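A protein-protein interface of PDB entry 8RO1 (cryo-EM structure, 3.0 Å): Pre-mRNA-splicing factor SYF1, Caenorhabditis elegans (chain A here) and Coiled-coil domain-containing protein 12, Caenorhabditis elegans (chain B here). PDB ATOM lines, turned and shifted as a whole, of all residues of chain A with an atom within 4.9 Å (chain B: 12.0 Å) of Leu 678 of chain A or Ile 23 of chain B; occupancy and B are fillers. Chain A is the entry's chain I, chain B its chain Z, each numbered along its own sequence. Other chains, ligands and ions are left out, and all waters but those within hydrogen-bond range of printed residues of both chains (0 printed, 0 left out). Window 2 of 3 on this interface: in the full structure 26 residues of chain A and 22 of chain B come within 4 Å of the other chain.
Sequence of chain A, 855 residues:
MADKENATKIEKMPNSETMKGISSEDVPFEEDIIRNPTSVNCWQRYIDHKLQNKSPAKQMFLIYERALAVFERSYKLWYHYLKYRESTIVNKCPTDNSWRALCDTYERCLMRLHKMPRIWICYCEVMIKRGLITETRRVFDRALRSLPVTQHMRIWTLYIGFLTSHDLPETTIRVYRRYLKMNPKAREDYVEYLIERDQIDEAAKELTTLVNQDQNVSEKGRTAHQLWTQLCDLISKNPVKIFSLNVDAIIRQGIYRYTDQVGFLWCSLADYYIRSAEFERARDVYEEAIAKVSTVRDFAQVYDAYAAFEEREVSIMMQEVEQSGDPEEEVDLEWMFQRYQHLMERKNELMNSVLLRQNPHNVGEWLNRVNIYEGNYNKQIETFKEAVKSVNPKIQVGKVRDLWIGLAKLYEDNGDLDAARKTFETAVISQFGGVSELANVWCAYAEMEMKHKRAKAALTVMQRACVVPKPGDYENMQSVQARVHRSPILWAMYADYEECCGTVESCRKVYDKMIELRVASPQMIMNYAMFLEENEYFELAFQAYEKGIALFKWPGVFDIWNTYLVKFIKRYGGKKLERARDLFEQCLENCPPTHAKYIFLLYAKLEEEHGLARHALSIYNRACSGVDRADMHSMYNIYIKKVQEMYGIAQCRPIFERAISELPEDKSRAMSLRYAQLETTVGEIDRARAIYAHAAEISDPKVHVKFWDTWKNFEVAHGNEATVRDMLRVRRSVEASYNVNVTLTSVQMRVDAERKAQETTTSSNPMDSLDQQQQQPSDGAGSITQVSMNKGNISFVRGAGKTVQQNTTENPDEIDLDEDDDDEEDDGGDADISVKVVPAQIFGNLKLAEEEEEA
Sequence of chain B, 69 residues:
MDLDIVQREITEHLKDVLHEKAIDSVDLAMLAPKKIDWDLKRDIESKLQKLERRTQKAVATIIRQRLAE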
ATOM      1  N   GLN A 644     -20.757 -29.402  22.774  1.00  0.00           N
ATOM      2  CA  GLN A 644     -19.644 -29.017  21.912  1.00  0.00           C
ATOM      3  C   GLN A 644     -18.818 -27.896  22.532  1.00  0.00           C
ATOM      4  O   GLN A 644     -17.584 -27.914  22.465  1.00  0.00           O
ATOM      5  CB  GLN A 644     -20.201 -28.617  20.542  1.00  0.00           C
ATOM      6  CG  GLN A 644     -19.233 -28.001  19.532  1.00  0.00           C
ATOM      7  CD  GLN A 644     -19.950 -27.549  18.276  1.00  0.00           C
ATOM      8  OE1 GLN A 644     -20.601 -28.348  17.602  1.00  0.00           O
ATOM      9  NE2 GLN A 644     -19.840 -26.265  17.953  1.00  0.00           N
ATOM     10  N   ILE A 649     -16.545 -31.810  20.058  1.00  0.00           N
ATOM     11  CA  ILE A 649     -17.384 -32.519  19.092  1.00  0.00           C
ATOM     12  C   ILE A 649     -17.330 -34.030  19.278  1.00  0.00           C
ATOM     13  O   ILE A 649     -18.278 -34.737  18.921  1.00  0.00           O
ATOM     14  CB  ILE A 649     -17.005 -32.118  17.651  1.00  0.00           C
ATOM     15  CG1 ILE A 649     -15.523 -32.403  17.352  1.00  0.00           C
ATOM     16  CG2 ILE A 649     -17.334 -30.650  17.430  1.00  0.00           C
ATOM     17  CD1 ILE A 649     -15.180 -32.337  15.895  1.00  0.00           C
ATOM     18  N   PHE A 656     -26.376 -36.529  18.582  1.00  0.00           N
ATOM     19  CA  PHE A 656     -26.788 -36.513  17.182  1.00  0.00           C
ATOM     20  C   PHE A 656     -27.565 -37.768  16.819  1.00  0.00           C
ATOM     21  O   PHE A 656     -28.616 -37.701  16.175  1.00  0.00           O
ATOM     22  CB  PHE A 656     -25.573 -36.388  16.268  1.00  0.00           C
ATOM     23  CG  PHE A 656     -25.107 -34.990  16.053  1.00  0.00           C
ATOM     24  CD1 PHE A 656     -25.764 -34.173  15.167  1.00  0.00           C
ATOM     25  CD2 PHE A 656     -24.001 -34.505  16.703  1.00  0.00           C
ATOM     26  CE1 PHE A 656     -25.337 -32.893  14.941  1.00  0.00           C
ATOM     27  CE2 PHE A 656     -23.571 -33.225  16.486  1.00  0.00           C
ATOM     28  CZ  PHE A 656     -24.235 -32.415  15.600  1.00  0.00           C
ATOM     29  N   ARG A 674     -26.183 -32.211   9.311  1.00  0.00           N
ATOM     30  CA  ARG A 674     -25.362 -31.650  10.381  1.00  0.00           C
ATOM     31  C   ARG A 674     -24.345 -32.660  10.896  1.00  0.00           C
ATOM     32  O   ARG A 674     -23.162 -32.346  11.045  1.00  0.00           O
ATOM     33  CB  ARG A 674     -26.272 -31.211  11.527  1.00  0.00           C
ATOM     34  CG  ARG A 674     -27.151 -30.009  11.233  1.00  0.00           C
ATOM     35  CD  ARG A 674     -26.572 -28.724  11.786  1.00  0.00           C
ATOM     36  NE  ARG A 674     -26.640 -28.730  13.249  1.00  0.00           N
ATOM     37  CZ  ARG A 674     -25.766 -28.176  14.083  1.00  0.00           C
ATOM     38  NH1 ARG A 674     -25.996 -28.241  15.390  1.00  0.00           N
ATOM     39  NH2 ARG A 674     -24.666 -27.575  13.655  1.00  0.00           N
ATOM     40  N   TYR A 675     -24.789 -33.887  11.151  1.00  0.00           N
ATOM     41  CA  TYR A 675     -23.893 -34.905  11.684  1.00  0.00           C
ATOM     42  C   TYR A 675     -22.854 -35.334  10.661  1.00  0.00           C
ATOM     43  O   TYR A 675     -21.710 -35.623  11.023  1.00  0.00           O
ATOM     44  CB  TYR A 675     -24.705 -36.098  12.190  1.00  0.00           C
ATOM     45  CG  TYR A 675     -23.957 -37.120  13.029  1.00  0.00           C
ATOM     46  CD1 TYR A 675     -22.880 -36.772  13.830  1.00  0.00           C
ATOM     47  CD2 TYR A 675     -24.368 -38.437  13.045  1.00  0.00           C
ATOM     48  CE1 TYR A 675     -22.219 -37.707  14.571  1.00  0.00           C
ATOM     49  CE2 TYR A 675     -23.716 -39.373  13.791  1.00  0.00           C
ATOM     50  CZ  TYR A 675     -22.649 -39.006  14.557  1.00  0.00           C
ATOM     51  OH  TYR A 675     -22.002 -39.951  15.316  1.00  0.00           O
ATOM     52  N   ALA A 676     -23.234 -35.401   9.388  1.00  0.00           N
ATOM     53  CA  ALA A 676     -22.268 -35.730   8.346  1.00  0.00           C
ATOM     54  C   ALA A 676     -21.187 -34.662   8.217  1.00  0.00           C
ATOM     55  O   ALA A 676     -20.027 -34.982   7.936  1.00  0.00           O
ATOM     56  CB  ALA A 676     -22.985 -35.919   7.015  1.00  0.00           C
ATOM     57  N   GLN A 677     -21.542 -33.390   8.403  1.00  0.00           N
ATOM     58  CA  GLN A 677     -20.532 -32.334   8.372  1.00  0.00           C
ATOM     59  C   GLN A 677     -19.477 -32.499   9.457  1.00  0.00           C
ATOM     60  O   GLN A 677     -18.293 -32.241   9.212  1.00  0.00           O
ATOM     61  CB  GLN A 677     -21.202 -30.972   8.516  1.00  0.00           C
ATOM     62  CG  GLN A 677     -21.914 -30.496   7.280  1.00  0.00           C
ATOM     63  CD  GLN A 677     -20.951 -29.982   6.232  1.00  0.00           C
ATOM     64  OE1 GLN A 677     -19.735 -30.113   6.370  1.00  0.00           O
ATOM     65  NE2 GLN A 677     -21.491 -29.385   5.177  1.00  0.00           N
ATOM     66  N   LEU A 678     -19.864 -32.930  10.657  1.00  0.00           N
ATOM     67  CA  LEU A 678     -18.853 -33.197  11.674  1.00  0.00           C
ATOM     68  C   LEU A 678     -17.965 -34.366  11.293  1.00  0.00           C
ATOM     69  O   LEU A 678     -16.737 -34.272  11.363  1.00  0.00           O
ATOM     70  CB  LEU A 678     -19.495 -33.474  13.031  1.00  0.00           C
ATOM     71  CG  LEU A 678     -20.112 -32.327  13.823  1.00  0.00           C
ATOM     72  CD1 LEU A 678     -20.600 -32.891  15.126  1.00  0.00           C
ATOM     73  CD2 LEU A 678     -19.121 -31.201  14.088  1.00  0.00           C
ATOM     74  N   GLU A 679     -18.562 -35.485  10.907  1.00  0.00           N
ATOM     75  CA  GLU A 679     -17.755 -36.654  10.591  1.00  0.00           C
ATOM     76  C   GLU A 679     -16.850 -36.424   9.385  1.00  0.00           C
ATOM     77  O   GLU A 679     -15.754 -36.990   9.328  1.00  0.00           O
ATOM     78  CB  GLU A 679     -18.668 -37.861  10.398  1.00  0.00           C
ATOM     79  CG  GLU A 679     -19.431 -38.291  11.670  1.00  0.00           C
ATOM     80  CD  GLU A 679     -18.580 -38.956  12.749  1.00  0.00           C
ATOM     81  OE1 GLU A 679     -17.397 -38.612  12.931  1.00  0.00           O
ATOM     82  OE2 GLU A 679     -19.122 -39.842  13.443  1.00  0.00           O
ATOM     83  N   THR A 680     -17.276 -35.608   8.416  1.00  0.00           N
ATOM     84  CA  THR A 680     -16.408 -35.335   7.272  1.00  0.00           C
ATOM     85  C   THR A 680     -15.315 -34.308   7.552  1.00  0.00           C
ATOM     86  O   THR A 680     -14.256 -34.376   6.918  1.00  0.00           O
ATOM     87  CB  THR A 680     -17.219 -34.845   6.071  1.00  0.00           C
ATOM     88  OG1 THR A 680     -18.048 -33.741   6.452  1.00  0.00           O
ATOM     89  CG2 THR A 680     -18.072 -35.958   5.503  1.00  0.00           C
ATOM     90  N   THR A 681     -15.516 -33.358   8.476  1.00  0.00           N
ATOM     91  CA  THR A 681     -14.398 -32.491   8.856  1.00  0.00           C
ATOM     92  C   THR A 681     -13.393 -33.222   9.742  1.00  0.00           C
ATOM     93  O   THR A 681     -12.185 -32.987   9.634  1.00  0.00           O
ATOM     94  CB  THR A 681     -14.912 -31.197   9.512  1.00  0.00           C
ATOM     95  OG1 THR A 681     -13.888 -30.198   9.440  1.00  0.00           O
ATOM     96  CG2 THR A 681     -15.356 -31.350  10.975  1.00  0.00           C
ATOM     97  N   VAL A 682     -13.865 -34.111  10.617  1.00  0.00           N
ATOM     98  CA  VAL A 682     -12.952 -34.956  11.379  1.00  0.00           C
ATOM     99  C   VAL A 682     -12.349 -36.023  10.472  1.00  0.00           C
ATOM    100  O   VAL A 682     -11.260 -36.531  10.757  1.00  0.00           O
ATOM    101  CB  VAL A 682     -13.695 -35.531  12.611  1.00  0.00           C
ATOM    102  CG1 VAL A 682     -12.825 -36.506  13.489  1.00  0.00           C
ATOM    103  CG2 VAL A 682     -14.223 -34.383  13.475  1.00  0.00           C
ATOM    104  N   GLY A 683     -13.006 -36.348   9.363  1.00  0.00           N
ATOM    105  CA  GLY A 683     -12.483 -37.302   8.412  1.00  0.00           C
ATOM    106  C   GLY A 683     -12.997 -38.710   8.588  1.00  0.00           C
ATOM    107  O   GLY A 683     -12.460 -39.629   7.961  1.00  0.00           O
ATOM    108  N   HIS B  19     -29.725 -21.908  18.029  1.00  0.00           N
ATOM    109  CA  HIS B  19     -29.412 -22.330  16.674  1.00  0.00           C
ATOM    110  C   HIS B  19     -27.899 -22.320  16.528  1.00  0.00           C
ATOM    111  O   HIS B  19     -27.187 -21.700  17.322  1.00  0.00           O
ATOM    112  CB  HIS B  19     -30.080 -21.424  15.640  1.00  0.00           C
ATOM    113  CG  HIS B  19     -29.616 -20.003  15.700  1.00  0.00           C
ATOM    114  ND1 HIS B  19     -28.645 -19.500  14.862  1.00  0.00           N
ATOM    115  CD2 HIS B  19     -29.989 -18.978  16.502  1.00  0.00           C
ATOM    116  CE1 HIS B  19     -28.440 -18.226  15.145  1.00  0.00           C
ATOM    117  NE2 HIS B  19     -29.243 -17.885  16.136  1.00  0.00           N
ATOM    118  N   GLU B  20     -27.414 -23.020  15.505  1.00  0.00           N
ATOM    119  CA  GLU B  20     -26.023 -22.912  15.088  1.00  0.00           C
ATOM    120  C   GLU B  20     -25.990 -22.875  13.570  1.00  0.00           C
ATOM    121  O   GLU B  20     -26.622 -23.703  12.909  1.00  0.00           O
ATOM    122  CB  GLU B  20     -25.183 -24.073  15.633  1.00  0.00           C
ATOM    123  CG  GLU B  20     -23.689 -23.929  15.392  1.00  0.00           C
ATOM    124  CD  GLU B  20     -22.884 -25.028  16.056  1.00  0.00           C
ATOM    125  OE1 GLU B  20     -23.288 -26.206  15.959  1.00  0.00           O
ATOM    126  OE2 GLU B  20     -21.848 -24.713  16.679  1.00  0.00           O
ATOM    127  N   LYS B  21     -25.250 -21.907  13.029  1.00  0.00           N
ATOM    128  CA  LYS B  21     -25.334 -21.613  11.604  1.00  0.00           C
ATOM    129  C   LYS B  21     -24.591 -22.649  10.765  1.00  0.00           C
ATOM    130  O   LYS B  21     -25.153 -23.209   9.819  1.00  0.00           O
ATOM    131  CB  LYS B  21     -24.765 -20.216  11.344  1.00  0.00           C
ATOM    132  CG  LYS B  21     -25.475 -19.075  12.095  1.00  0.00           C
ATOM    133  CD  LYS B  21     -26.957 -18.895  11.762  1.00  0.00           C
ATOM    134  CE  LYS B  21     -27.195 -18.517  10.307  1.00  0.00           C
ATOM    135  NZ  LYS B  21     -28.642 -18.318  10.025  1.00  0.00           N
ATOM    136  N   ALA B  22     -23.331 -22.919  11.100  1.00  0.00           N
ATOM    137  CA  ALA B  22     -22.539 -23.889  10.358  1.00  0.00           C
ATOM    138  C   ALA B  22     -21.336 -24.286  11.198  1.00  0.00           C
ATOM    139  O   ALA B  22     -20.987 -23.609  12.168  1.00  0.00           O
ATOM    140  CB  ALA B  22     -22.088 -23.332   9.003  1.00  0.00           C
ATOM    141  N   ILE B  23     -20.715 -25.399  10.818  1.00  0.00           N
ATOM    142  CA  ILE B  23     -19.385 -25.752  11.302  1.00  0.00           C
ATOM    143  C   ILE B  23     -18.591 -26.337  10.142  1.00  0.00           C
ATOM    144  O   ILE B  23     -19.101 -27.181   9.398  1.00  0.00           O
ATOM    145  CB  ILE B  23     -19.456 -26.718  12.509  1.00  0.00           C
ATOM    146  CG1 ILE B  23     -18.076 -26.925  13.156  1.00  0.00           C
ATOM    147  CG2 ILE B  23     -20.097 -28.065  12.138  1.00  0.00           C
ATOM    148  CD1 ILE B  23     -17.453 -25.660  13.751  1.00  0.00           C
ATOM    149  N   ASP B  24     -17.349 -25.876   9.981  1.00  0.00           N
ATOM    150  CA  ASP B  24     -16.560 -26.178   8.790  1.00  0.00           C
ATOM    151  C   ASP B  24     -15.064 -26.047   9.063  1.00  0.00           C
ATOM    152  O   ASP B  24     -14.296 -25.662   8.175  1.00  0.00           O
ATOM    153  CB  ASP B  24     -16.976 -25.253   7.640  1.00  0.00           C
ATOM    154  CG  ASP B  24     -16.572 -25.783   6.268  1.00  0.00           C
ATOM    155  OD1 ASP B  24     -16.245 -26.982   6.139  1.00  0.00           O
ATOM    156  OD2 ASP B  24     -16.580 -24.985   5.306  1.00  0.00           O
ATOM    157  N   SER B  25     -14.640 -26.353  10.283  1.00  0.00           N
ATOM    158  CA  SER B  25     -13.228 -26.317  10.639  1.00  0.00           C
ATOM    159  C   SER B  25     -13.055 -27.089  11.937  1.00  0.00           C
ATOM    160  O   SER B  25     -14.025 -27.390  12.636  1.00  0.00           O
ATOM    161  CB  SER B  25     -12.721 -24.878  10.772  1.00  0.00           C
ATOM    162  OG  SER B  25     -12.345 -24.354   9.511  1.00  0.00           O
ATOM    163  N   VAL B  26     -11.801 -27.400  12.257  1.00  0.00           N
ATOM    164  CA  VAL B  26     -11.456 -27.934  13.568  1.00  0.00           C
ATOM    165  C   VAL B  26     -10.062 -27.457  13.939  1.00  0.00           C
ATOM    166  O   VAL B  26      -9.236 -27.156  13.075  1.00  0.00           O
ATOM    167  CB  VAL B  26     -11.577 -29.483  13.575  1.00  0.00           C
ATOM    168  CG1 VAL B  26     -10.397 -30.161  12.857  1.00  0.00           C
ATOM    169  CG2 VAL B  26     -11.721 -30.032  15.000  1.00  0.00           C
ATOM    170  N   ASP B  27      -9.811 -27.382  15.244  1.00  0.00           N
ATOM    171  CA  ASP B  27      -8.509 -26.995  15.763  1.00  0.00           C
ATOM    172  C   ASP B  27      -8.293 -27.655  17.117  1.00  0.00           C
ATOM    173  O   ASP B  27      -9.199 -28.276  17.679  1.00  0.00           O
ATOM    174  CB  ASP B  27      -8.384 -25.460  15.822  1.00  0.00           C
ATOM    175  CG  ASP B  27      -9.426 -24.789  16.734  1.00  0.00           C
ATOM    176  OD1 ASP B  27      -9.782 -25.300  17.817  1.00  0.00           O
ATOM    177  OD2 ASP B  27      -9.905 -23.704  16.344  1.00  0.00           O
ATOM    178  N   LEU B  28      -7.059 -27.529  17.617  1.00  0.00           N
ATOM    179  CA  LEU B  28      -6.662 -28.216  18.844  1.00  0.00           C
ATOM    180  C   LEU B  28      -7.544 -27.824  20.022  1.00  0.00           C
ATOM    181  O   LEU B  28      -7.857 -28.660  20.877  1.00  0.00           O
ATOM    182  CB  LEU B  28      -5.189 -27.941  19.165  1.00  0.00           C
ATOM    183  CG  LEU B  28      -4.047 -28.539  18.320  1.00  0.00           C
ATOM    184  CD1 LEU B  28      -4.170 -30.062  18.184  1.00  0.00           C
ATOM    185  CD2 LEU B  28      -3.916 -27.903  16.938  1.00  0.00           C
ATOM    186  N   ALA B  29      -7.960 -26.559  20.083  1.00  0.00           N
ATOM    187  CA  ALA B  29      -8.871 -26.146  21.143  1.00  0.00           C
ATOM    188  C   ALA B  29     -10.257 -26.743  20.950  1.00  0.00           C
ATOM    189  O   ALA B  29     -10.885 -27.182  21.920  1.00  0.00           O
ATOM    190  CB  ALA B  29      -8.947 -24.621  21.198  1.00  0.00           C
ATOM    191  N   MET B  30     -10.758 -26.764  19.712  1.00  0.00           N
ATOM    192  CA  MET B  30     -12.125 -27.222  19.494  1.00  0.00           C
ATOM    193  C   MET B  30     -12.275 -28.709  19.787  1.00  0.00           C
ATOM    194  O   MET B  30     -13.364 -29.156  20.162  1.00  0.00           O
ATOM    195  CB  MET B  30     -12.542 -26.921  18.051  1.00  0.00           C
ATOM    196  CG  MET B  30     -13.929 -27.424  17.646  1.00  0.00           C
ATOM    197  SD  MET B  30     -14.348 -27.019  15.946  1.00  0.00           S
ATOM    198  CE  MET B  30     -15.617 -28.249  15.664  1.00  0.00           C
ATOM    199  N   LEU B  31     -11.209 -29.491  19.608  1.00  0.00           N
ATOM    200  CA  LEU B  31     -11.257 -30.907  19.956  1.00  0.00           C
ATOM    201  C   LEU B  31     -11.519 -31.133  21.440  1.00  0.00           C
ATOM    202  O   LEU B  31     -12.115 -32.150  21.813  1.00  0.00           O
ATOM    203  CB  LEU B  31      -9.953 -31.586  19.540  1.00  0.00           C
ATOM    204  CG  LEU B  31      -9.657 -31.624  18.038  1.00  0.00           C
ATOM    205  CD1 LEU B  31      -8.209 -32.023  17.795  1.00  0.00           C
ATOM    206  CD2 LEU B  31     -10.603 -32.559  17.300  1.00  0.00           C
ATOM    207  N   ALA B  32     -11.083 -30.214  22.299  1.00  0.00           N
ATOM    208  CA  ALA B  32     -11.255 -30.369  23.738  1.00  0.00           C
ATOM    209  C   ALA B  32     -11.129 -29.017  24.427  1.00  0.00           C
ATOM    210  O   ALA B  32     -10.101 -28.736  25.054  1.00  0.00           O
ATOM    211  CB  ALA B  32     -10.222 -31.345  24.300  1.00  0.00           C
ATOM    212  N   PRO B  33     -12.139 -28.150  24.337  1.00  0.00           N
ATOM    213  CA  PRO B  33     -11.941 -26.773  24.802  1.00  0.00           C
ATOM    214  C   PRO B  33     -11.914 -26.628  26.312  1.00  0.00           C
ATOM    215  O   PRO B  33     -11.256 -25.707  26.810  1.00  0.00           O
ATOM    216  CB  PRO B  33     -13.133 -26.026  24.193  1.00  0.00           C
ATOM    217  CG  PRO B  33     -14.171 -27.055  24.017  1.00  0.00           C
ATOM    218  CD  PRO B  33     -13.458 -28.333  23.712  1.00  0.00           C
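Gln 644 of chain A touches Pro 33 of chain B (O to CG, 3.8 Å). Met 30 of chain B touches Ile 649 of chain A. CD2 of Leu 678 of chain A touches CG2 of Ile 23 of chain B, 3.8 Å away.
Leu 678 of chain A touches just one residue of chain B: Ile 23 (3.8 Å). Ile 23 of chain B touches just one residue of chain A: Leu 678 (3.8 Å). Of chain B, only Met 30 comes within 4 Å of Ile 649 of chain A. No residue of chain B comes within 4 Å of Tyr 675 of chain A. No residue of chain B comes within 4 Å of Ala 676 of chain A. No residue of chain B comes within 4 Å of Gln 677 of chain A. No residue of chain B comes within 4 Å of Glu 679 of chain A. No residue of chain B comes within 4 Å of Thr 680 of chain A. No residue of chain B comes within 4 Å of Val 682 of chain A. Gly 683 of chain A touches none of the printed residues of chain B. Printed residues of chain A within 4 Å of Glu 20 of chain B: Gln 644 and Arg 674. Of the printed residues of chain A, Met 30 of chain B touches Ile 649 (3.4 Å). Printed residues of chain A within 4 Å of Pro 33 of chain B: Gln 644. Of the printed residues of chain B, Gln 644 of chain A touches Glu 20 (2.8 Å) and Pro 33 (3.8 Å). Asp 27 of chain B touches none of the printed residues of chain A. The nearest residue of chain B that does not touch Leu 678 of chain A is Met 30 of chain B (4.8 Å). The nearest residue of chain A that does not touch Ile 23 of chain B is Gln 677 of chain A (4.3 Å).
OD1 of Asp 27 of chain B sits at hydrogen-bond distance from N of Met 30 of chain B (2.6 Å).
Of the 15 printed residues of chain B, 4 touch a printed residue of chain A. Printed residues of chain B that touch a printed residue of chain A: Glu 20, Ile 23, Met 30 and Pro 33. Among the printed residues, 5 pairs touch across the chains. Among the printed residues, Asp or Glu carboxylates within 4 Å of a Lys or Arg side-chain nitrogen of the other chain: Arg 674 of chain A with Glu 20 of chain B (3.0 Å).
OE2 of Glu 20 of chain B sits at hydrogen-bond distance from NE2 of Gln 644 of chain A, at 2.8 Å. The guanidinium group (NH2) of Arg 674 of chain A is in salt-bridge range of the side-chain carboxylate (OE1) of Glu 20 of chain B, 3.0 Å away.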
